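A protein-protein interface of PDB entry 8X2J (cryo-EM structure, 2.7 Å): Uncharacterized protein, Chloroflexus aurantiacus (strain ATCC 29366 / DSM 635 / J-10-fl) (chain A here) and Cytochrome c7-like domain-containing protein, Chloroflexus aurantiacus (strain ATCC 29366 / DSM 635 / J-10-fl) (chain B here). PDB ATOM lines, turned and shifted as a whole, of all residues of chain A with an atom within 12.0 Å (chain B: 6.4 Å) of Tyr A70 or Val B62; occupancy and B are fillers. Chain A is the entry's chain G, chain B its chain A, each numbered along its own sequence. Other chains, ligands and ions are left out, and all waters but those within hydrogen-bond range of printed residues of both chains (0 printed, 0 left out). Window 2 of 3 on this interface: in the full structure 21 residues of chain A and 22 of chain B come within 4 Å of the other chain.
Of the printed residues of chain B, Val A65 touches Val B61. Gly A67 touches none of the printed residues of chain B. Tyr A70 touches five residues of chain B. Of the printed residues of chain B, Arg A71 touches Asn B60 and Asp B185. No residue of chain A comes within 4 Å of Leu B57. No residue of chain A comes within 4 Å of His B58. Val B59 touches just one residue of chain A: Tyr A70. Asn B60 touches just these residues of chain A: Thr A69, Tyr A70 and Arg A71. Val B61 touches just these residues of chain A: Val A65, Asn A68, Thr A69 and Tyr A70. Of chain A, only Tyr A70 (3.6 Å) comes within 4 Å of Val B62. No residue of chain A comes within 4 Å of Ile B64. The nearest residue of chain A that does not touch Val B62 is Thr A69 (5.9 Å).
CG1 of Val A65 touches CG2 of Val B61, 3.7 Å away. Val B61 touches Asn A68. Thr A69 touches Asn B60. Thr A69 touches Val B61. Val B59 touches Tyr A70 (O to CE1, 3.3 Å). Tyr A70 touches Asn B60. Tyr A70 touches Val B62 (CB to O, 3.6 Å). Tyr A70 touches Gly B63 (CG to CA, 3.4 Å).
N of Val B62 lies within hydrogen-bond range of O of Leu B57 (2.8 Å). The backbone carbonyl oxygen (O) of His B58 is in hydrogen-bond range of the backbone NH (N) of Gly B63 (3.3 Å). OG1 of Thr A69 sits close to N of Arg A71 (3.5 Å). O of Thr A69 sits at hydrogen-bond distance from OG1 of Thr A72, at 3.3 Å. ND2 of Asn A75 sits close to O of Arg A71.
Hydrophobic or aromatic side chains of chain A that line the printed part of chain B: Val A65 and Tyr A70. Hydrophobic or aromatic side chains of chain B that line the printed part of chain A: Val B61. Among the printed residues, Asp or Glu carboxylates within 4 Å of a Lys or Arg side-chain nitrogen of the other chain: Arg A71 with Asp B185 (3.2 Å).
OD1 of Asn B60 is in hydrogen-bond range of NH2 of Arg A71 (3.2 Å). O of Val B61 is in hydrogen-bond range of N of Tyr A70 (3.2 Å). NH2 of Arg A71 is in salt-bridge range of OD1 of Asp B185, at 3.2 Å.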
ATOM      1  N   PRO A  64       7.070  -7.348  28.320  1.00  0.00           N
ATOM      2  CA  PRO A  64       6.041  -6.372  27.949  1.00  0.00           C
ATOM      3  C   PRO A  64       6.570  -4.946  28.006  1.00  0.00           C
ATOM      4  O   PRO A  64       7.521  -4.629  28.723  1.00  0.00           O
ATOM      5  CB  PRO A  64       4.939  -6.596  28.993  1.00  0.00           C
ATOM      6  CG  PRO A  64       5.242  -7.930  29.608  1.00  0.00           C
ATOM      7  CD  PRO A  64       6.726  -8.065  29.558  1.00  0.00           C
ATOM      8  N   VAL A  65       5.931  -4.081  27.221  1.00  0.00           N
ATOM      9  CA  VAL A  65       6.319  -2.676  27.168  1.00  0.00           C
ATOM     10  C   VAL A  65       5.823  -1.978  28.427  1.00  0.00           C
ATOM     11  O   VAL A  65       4.616  -1.927  28.692  1.00  0.00           O
ATOM     12  CB  VAL A  65       5.767  -2.004  25.906  1.00  0.00           C
ATOM     13  CG1 VAL A  65       6.109  -0.527  25.907  1.00  0.00           C
ATOM     14  CG2 VAL A  65       6.311  -2.688  24.663  1.00  0.00           C
ATOM     15  N   THR A  66       6.752  -1.435  29.209  1.00  0.00           N
ATOM     16  CA  THR A  66       6.438  -0.821  30.491  1.00  0.00           C
ATOM     17  C   THR A  66       6.401   0.702  30.430  1.00  0.00           C
ATOM     18  O   THR A  66       6.289   1.349  31.476  1.00  0.00           O
ATOM     19  CB  THR A  66       7.447  -1.272  31.550  1.00  0.00           C
ATOM     20  OG1 THR A  66       7.118  -0.673  32.810  1.00  0.00           O
ATOM     21  CG2 THR A  66       8.856  -0.861  31.149  1.00  0.00           C
ATOM     22  N   GLY A  67       6.490   1.288  29.238  1.00  0.00           N
ATOM     23  CA  GLY A  67       6.515   2.732  29.120  1.00  0.00           C
ATOM     24  C   GLY A  67       5.380   3.299  28.293  1.00  0.00           C
ATOM     25  O   GLY A  67       4.405   2.600  28.002  1.00  0.00           O
ATOM     26  N   ASN A  68       5.495   4.572  27.919  1.00  0.00           N
ATOM     27  CA  ASN A  68       4.486   5.205  27.082  1.00  0.00           C
ATOM     28  C   ASN A  68       4.552   4.656  25.665  1.00  0.00           C
ATOM     29  O   ASN A  68       5.631   4.372  25.140  1.00  0.00           O
ATOM     30  CB  ASN A  68       4.680   6.721  27.068  1.00  0.00           C
ATOM     31  CG  ASN A  68       4.745   7.314  28.461  1.00  0.00           C
ATOM     32  OD1 ASN A  68       4.192   6.760  29.411  1.00  0.00           O
ATOM     33  ND2 ASN A  68       5.425   8.447  28.590  1.00  0.00           N
ATOM     34  N   THR A  69       3.387   4.494  25.049  1.00  0.00           N
ATOM     35  CA  THR A  69       3.264   3.919  23.717  1.00  0.00           C
ATOM     36  C   THR A  69       2.552   4.901  22.790  1.00  0.00           C
ATOM     37  O   THR A  69       2.143   5.993  23.190  1.00  0.00           O
ATOM     38  CB  THR A  69       2.504   2.589  23.758  1.00  0.00           C
ATOM     39  OG1 THR A  69       1.210   2.795  24.337  1.00  0.00           O
ATOM     40  CG2 THR A  69       3.258   1.562  24.581  1.00  0.00           C
ATOM     41  N   TYR A  70       2.409   4.483  21.531  1.00  0.00           N
ATOM     42  CA  TYR A  70       1.659   5.230  20.530  1.00  0.00           C
ATOM     43  C   TYR A  70       0.154   5.130  20.720  1.00  0.00           C
ATOM     44  O   TYR A  70      -0.582   5.891  20.080  1.00  0.00           O
ATOM     45  CB  TYR A  70       2.008   4.726  19.132  1.00  0.00           C
ATOM     46  CG  TYR A  70       1.262   3.467  18.734  1.00  0.00           C
ATOM     47  CD1 TYR A  70       1.543   2.247  19.339  1.00  0.00           C
ATOM     48  CD2 TYR A  70       0.296   3.493  17.735  1.00  0.00           C
ATOM     49  CE1 TYR A  70       0.874   1.097  18.976  1.00  0.00           C
ATOM     50  CE2 TYR A  70      -0.380   2.347  17.367  1.00  0.00           C
ATOM     51  CZ  TYR A  70      -0.086   1.153  17.990  1.00  0.00           C
ATOM     52  OH  TYR A  70      -0.754   0.009  17.625  1.00  0.00           O
ATOM     53  N   ARG A  71      -0.308   4.194  21.553  1.00  0.00           N
ATOM     54  CA  ARG A  71      -1.736   3.962  21.719  1.00  0.00           C
ATOM     55  C   ARG A  71      -2.430   5.144  22.379  1.00  0.00           C
ATOM     56  O   ARG A  71      -3.571   5.452  22.027  1.00  0.00           O
ATOM     57  CB  ARG A  71      -1.967   2.687  22.528  1.00  0.00           C
ATOM     58  CG  ARG A  71      -1.424   1.434  21.864  1.00  0.00           C
ATOM     59  CD  ARG A  71      -1.733   0.194  22.683  1.00  0.00           C
ATOM     60  NE  ARG A  71      -1.708  -1.015  21.868  1.00  0.00           N
ATOM     61  CZ  ARG A  71      -0.621  -1.736  21.631  1.00  0.00           C
ATOM     62  NH1 ARG A  71       0.556  -1.400  22.134  1.00  0.00           N
ATOM     63  NH2 ARG A  71      -0.718  -2.824  20.872  1.00  0.00           N
ATOM     64  N   THR A  72      -1.757   5.825  23.313  1.00  0.00           N
ATOM     65  CA  THR A  72      -2.334   7.016  23.932  1.00  0.00           C
ATOM     66  C   THR A  72      -2.514   8.140  22.918  1.00  0.00           C
ATOM     67  O   THR A  72      -3.567   8.790  22.891  1.00  0.00           O
ATOM     68  CB  THR A  72      -1.461   7.481  25.097  1.00  0.00           C
ATOM     69  OG1 THR A  72      -0.185   7.904  24.603  1.00  0.00           O
ATOM     70  CG2 THR A  72      -1.262   6.354  26.095  1.00  0.00           C
ATOM     71  N   TYR A  73      -1.512   8.356  22.056  1.00  0.00           N
ATOM     72  CA  TYR A  73      -1.608   9.374  21.012  1.00  0.00           C
ATOM     73  C   TYR A  73      -2.700   9.042  20.004  1.00  0.00           C
ATOM     74  O   TYR A  73      -3.484   9.918  19.617  1.00  0.00           O
ATOM     75  CB  TYR A  73      -0.268   9.518  20.288  1.00  0.00           C
ATOM     76  CG  TYR A  73       0.814  10.204  21.084  1.00  0.00           C
ATOM     77  CD1 TYR A  73       0.816  11.583  21.242  1.00  0.00           C
ATOM     78  CD2 TYR A  73       1.843   9.473  21.662  1.00  0.00           C
ATOM     79  CE1 TYR A  73       1.808  12.215  21.965  1.00  0.00           C
ATOM     80  CE2 TYR A  73       2.840  10.097  22.385  1.00  0.00           C
ATOM     81  CZ  TYR A  73       2.817  11.468  22.533  1.00  0.00           C
ATOM     82  OH  TYR A  73       3.806  12.095  23.252  1.00  0.00           O
ATOM     83  N   VAL A  74      -2.773   7.775  19.584  1.00  0.00           N
ATOM     84  CA  VAL A  74      -3.759   7.354  18.592  1.00  0.00           C
ATOM     85  C   VAL A  74      -5.173   7.451  19.157  1.00  0.00           C
ATOM     86  O   VAL A  74      -6.085   7.956  18.490  1.00  0.00           O
ATOM     87  CB  VAL A  74      -3.420   5.934  18.096  1.00  0.00           C
ATOM     88  CG1 VAL A  74      -4.617   5.256  17.456  1.00  0.00           C
ATOM     89  CG2 VAL A  74      -2.270   5.995  17.109  1.00  0.00           C
ATOM     90  N   ASN A  75      -5.368   7.018  20.408  1.00  0.00           N
ATOM     91  CA  ASN A  75      -6.688   7.082  21.030  1.00  0.00           C
ATOM     92  C   ASN A  75      -7.119   8.520  21.294  1.00  0.00           C
ATOM     93  O   ASN A  75      -8.292   8.860  21.097  1.00  0.00           O
ATOM     94  CB  ASN A  75      -6.690   6.273  22.325  1.00  0.00           C
ATOM     95  CG  ASN A  75      -6.596   4.782  22.079  1.00  0.00           C
ATOM     96  OD1 ASN A  75      -6.641   4.326  20.937  1.00  0.00           O
ATOM     97  ND2 ASN A  75      -6.449   4.013  23.151  1.00  0.00           N
ATOM     98  N   ASP A  76      -6.185   9.384  21.715  1.00  0.00           N
ATOM     99  CA  ASP A  76      -6.513  10.791  21.923  1.00  0.00           C
ATOM    100  C   ASP A  76      -6.855  11.485  20.609  1.00  0.00           C
ATOM    101  O   ASP A  76      -7.794  12.289  20.556  1.00  0.00           O
ATOM    102  CB  ASP A  76      -5.353  11.502  22.619  1.00  0.00           C
ATOM    103  CG  ASP A  76      -5.291  11.200  24.101  1.00  0.00           C
ATOM    104  OD1 ASP A  76      -6.229  10.558  24.619  1.00  0.00           O
ATOM    105  OD2 ASP A  76      -4.302  11.602  24.750  1.00  0.00           O
ATOM    106  N   ALA A  77      -6.127  11.167  19.534  1.00  0.00           N
ATOM    107  CA  ALA A  77      -6.414  11.780  18.240  1.00  0.00           C
ATOM    108  C   ALA A  77      -7.729  11.275  17.657  1.00  0.00           C
ATOM    109  O   ALA A  77      -8.468  12.041  17.028  1.00  0.00           O
ATOM    110  CB  ALA A  77      -5.261  11.521  17.274  1.00  0.00           C
ATOM    111  N   ARG A  78      -8.048   9.993  17.863  1.00  0.00           N
ATOM    112  CA  ARG A  78      -9.314   9.465  17.365  1.00  0.00           C
ATOM    113  C   ARG A  78     -10.495   9.960  18.192  1.00  0.00           C
ATOM    114  O   ARG A  78     -11.607  10.079  17.666  1.00  0.00           O
ATOM    115  CB  ARG A  78      -9.278   7.938  17.346  1.00  0.00           C
ATOM    116  CG  ARG A  78      -8.427   7.355  16.229  1.00  0.00           C
ATOM    117  CD  ARG A  78      -8.648   5.860  16.096  1.00  0.00           C
ATOM    118  NE  ARG A  78      -7.480   5.174  15.556  1.00  0.00           N
ATOM    119  CZ  ARG A  78      -7.207   5.055  14.264  1.00  0.00           C
ATOM    120  NH1 ARG A  78      -7.991   5.582  13.339  1.00  0.00           N
ATOM    121  NH2 ARG A  78      -6.119   4.387  13.890  1.00  0.00           N
ATOM    122  N   THR A  79     -10.283  10.242  19.481  1.00  0.00           N
ATOM    123  CA  THR A  79     -11.327  10.882  20.273  1.00  0.00           C
ATOM    124  C   THR A  79     -11.515  12.339  19.863  1.00  0.00           C
ATOM    125  O   THR A  79     -12.644  12.839  19.826  1.00  0.00           O
ATOM    126  CB  THR A  79     -10.997  10.782  21.762  1.00  0.00           C
ATOM    127  OG1 THR A  79     -10.500   9.470  22.054  1.00  0.00           O
ATOM    128  CG2 THR A  79     -12.235  11.045  22.605  1.00  0.00           C
ATOM    129  N   GLN B  56       9.237  -4.988  18.063  1.00  0.00           N
ATOM    130  CA  GLN B  56       8.452  -4.712  19.263  1.00  0.00           C
ATOM    131  C   GLN B  56       8.485  -3.235  19.615  1.00  0.00           C
ATOM    132  O   GLN B  56       7.438  -2.623  19.840  1.00  0.00           O
ATOM    133  CB  GLN B  56       8.960  -5.549  20.435  1.00  0.00           C
ATOM    134  CG  GLN B  56       8.246  -5.256  21.741  1.00  0.00           C
ATOM    135  CD  GLN B  56       8.864  -5.972  22.920  1.00  0.00           C
ATOM    136  OE1 GLN B  56      10.000  -5.697  23.301  1.00  0.00           O
ATOM    137  NE2 GLN B  56       8.115  -6.895  23.509  1.00  0.00           N
ATOM    138  N   LEU B  57       9.678  -2.637  19.602  1.00  0.00           N
ATOM    139  CA  LEU B  57       9.802  -1.200  19.815  1.00  0.00           C
ATOM    140  C   LEU B  57       9.112  -0.418  18.705  1.00  0.00           C
ATOM    141  O   LEU B  57       8.231   0.408  18.972  1.00  0.00           O
ATOM    142  CB  LEU B  57      11.276  -0.814  19.909  1.00  0.00           C
ATOM    143  CG  LEU B  57      11.595   0.631  20.288  1.00  0.00           C
ATOM    144  CD1 LEU B  57      11.239   0.909  21.737  1.00  0.00           C
ATOM    145  CD2 LEU B  57      13.059   0.901  20.042  1.00  0.00           C
ATOM    146  N   HIS B  58       9.432  -0.740  17.450  1.00  0.00           N
ATOM    147  CA  HIS B  58       8.978   0.060  16.318  1.00  0.00           C
ATOM    148  C   HIS B  58       7.487  -0.058  16.031  1.00  0.00           C
ATOM    149  O   HIS B  58       6.958   0.789  15.308  1.00  0.00           O
ATOM    150  CB  HIS B  58       9.772  -0.316  15.070  1.00  0.00           C
ATOM    151  CG  HIS B  58      11.188   0.159  15.101  1.00  0.00           C
ATOM    152  ND1 HIS B  58      12.171  -0.481  15.823  1.00  0.00           N
ATOM    153  CD2 HIS B  58      11.785   1.220  14.510  1.00  0.00           C
ATOM    154  CE1 HIS B  58      13.314   0.162  15.673  1.00  0.00           C
ATOM    155  NE2 HIS B  58      13.108   1.197  14.878  1.00  0.00           N
ATOM    156  N   VAL B  59       6.790  -1.057  16.568  1.00  0.00           N
ATOM    157  CA  VAL B  59       5.344  -1.170  16.396  1.00  0.00           C
ATOM    158  C   VAL B  59       4.602  -0.911  17.706  1.00  0.00           C
ATOM    159  O   VAL B  59       3.715  -0.059  17.763  1.00  0.00           O
ATOM    160  CB  VAL B  59       4.952  -2.532  15.785  1.00  0.00           C
ATOM    161  CG1 VAL B  59       3.458  -2.566  15.556  1.00  0.00           C
ATOM    162  CG2 VAL B  59       5.683  -2.757  14.476  1.00  0.00           C
ATOM    163  N   ASN B  60       4.933  -1.652  18.767  1.00  0.00           N
ATOM    164  CA  ASN B  60       4.196  -1.502  20.013  1.00  0.00           C
ATOM    165  C   ASN B  60       4.530  -0.208  20.744  1.00  0.00           C
ATOM    166  O   ASN B  60       3.728   0.235  21.572  1.00  0.00           O
ATOM    167  CB  ASN B  60       4.466  -2.696  20.928  1.00  0.00           C
ATOM    168  CG  ASN B  60       3.410  -3.771  20.809  1.00  0.00           C
ATOM    169  OD1 ASN B  60       2.361  -3.562  20.201  1.00  0.00           O
ATOM    170  ND2 ASN B  60       3.681  -4.932  21.388  1.00  0.00           N
ATOM    171  N   VAL B  61       5.677   0.412  20.467  1.00  0.00           N
ATOM    172  CA  VAL B  61       6.081   1.649  21.130  1.00  0.00           C
ATOM    173  C   VAL B  61       6.016   2.831  20.172  1.00  0.00           C
ATOM    174  O   VAL B  61       5.303   3.803  20.422  1.00  0.00           O
ATOM    175  CB  VAL B  61       7.488   1.511  21.754  1.00  0.00           C
ATOM    176  CG1 VAL B  61       7.794   2.715  22.626  1.00  0.00           C
ATOM    177  CG2 VAL B  61       7.591   0.226  22.549  1.00  0.00           C
ATOM    178  N   VAL B  62       6.765   2.767  19.069  1.00  0.00           N
ATOM    179  CA  VAL B  62       6.811   3.873  18.117  1.00  0.00           C
ATOM    180  C   VAL B  62       5.492   3.991  17.363  1.00  0.00           C
ATOM    181  O   VAL B  62       4.968   5.095  17.172  1.00  0.00           O
ATOM    182  CB  VAL B  62       8.005   3.687  17.164  1.00  0.00           C
ATOM    183  CG1 VAL B  62       8.155   4.883  16.261  1.00  0.00           C
ATOM    184  CG2 VAL B  62       9.278   3.462  17.958  1.00  0.00           C
ATOM    185  N   GLY B  63       4.931   2.865  16.936  1.00  0.00           N
ATOM    186  CA  GLY B  63       3.630   2.872  16.306  1.00  0.00           C
ATOM    187  C   GLY B  63       3.635   2.933  14.803  1.00  0.00           C
ATOM    188  O   GLY B  63       2.675   3.440  14.211  1.00  0.00           O
ATOM    189  N   ILE B  64       4.681   2.433  14.165  1.00  0.00           N
ATOM    190  CA  ILE B  64       4.782   2.475  12.714  1.00  0.00           C
ATOM    191  C   ILE B  64       3.870   1.410  12.121  1.00  0.00           C
ATOM    192  O   ILE B  64       3.870   0.257  12.567  1.00  0.00           O
ATOM    193  CB  ILE B  64       6.237   2.279  12.268  1.00  0.00           C
ATOM    194  CG1 ILE B  64       7.173   3.178  13.073  1.00  0.00           C
ATOM    195  CG2 ILE B  64       6.385   2.607  10.820  1.00  0.00           C
ATOM    196  CD1 ILE B  64       8.603   2.693  13.094  1.00  0.00           C
ATOM    197  N   ASN B 183      -4.511  -5.001  11.803  1.00  0.00           N
ATOM    198  CA  ASN B 183      -4.704  -4.806  13.232  1.00  0.00           C
ATOM    199  C   ASN B 183      -4.075  -5.970  13.983  1.00  0.00           C
ATOM    200  O   ASN B 183      -4.521  -7.115  13.854  1.00  0.00           O
ATOM    201  CB  ASN B 183      -6.191  -4.692  13.556  1.00  0.00           C
ATOM    202  CG  ASN B 183      -6.446  -4.084  14.918  1.00  0.00           C
ATOM    203  OD1 ASN B 183      -5.755  -3.156  15.337  1.00  0.00           O
ATOM    204  ND2 ASN B 183      -7.450  -4.600  15.615  1.00  0.00           N
ATOM    205  N   ASP B 185      -4.096  -6.178  17.214  1.00  0.00           N
ATOM    206  CA  ASP B 185      -4.876  -6.380  18.424  1.00  0.00           C
ATOM    207  C   ASP B 185      -6.123  -7.217  18.187  1.00  0.00           C
ATOM    208  O   ASP B 185      -6.869  -7.472  19.138  1.00  0.00           O
ATOM    209  CB  ASP B 185      -5.271  -5.026  19.022  1.00  0.00           C
ATOM    210  CG  ASP B 185      -4.071  -4.165  19.354  1.00  0.00           C
ATOM    211  OD1 ASP B 185      -3.000  -4.728  19.660  1.00  0.00           O
ATOM    212  OD2 ASP B 185      -4.197  -2.924  19.305  1.00  0.00           O
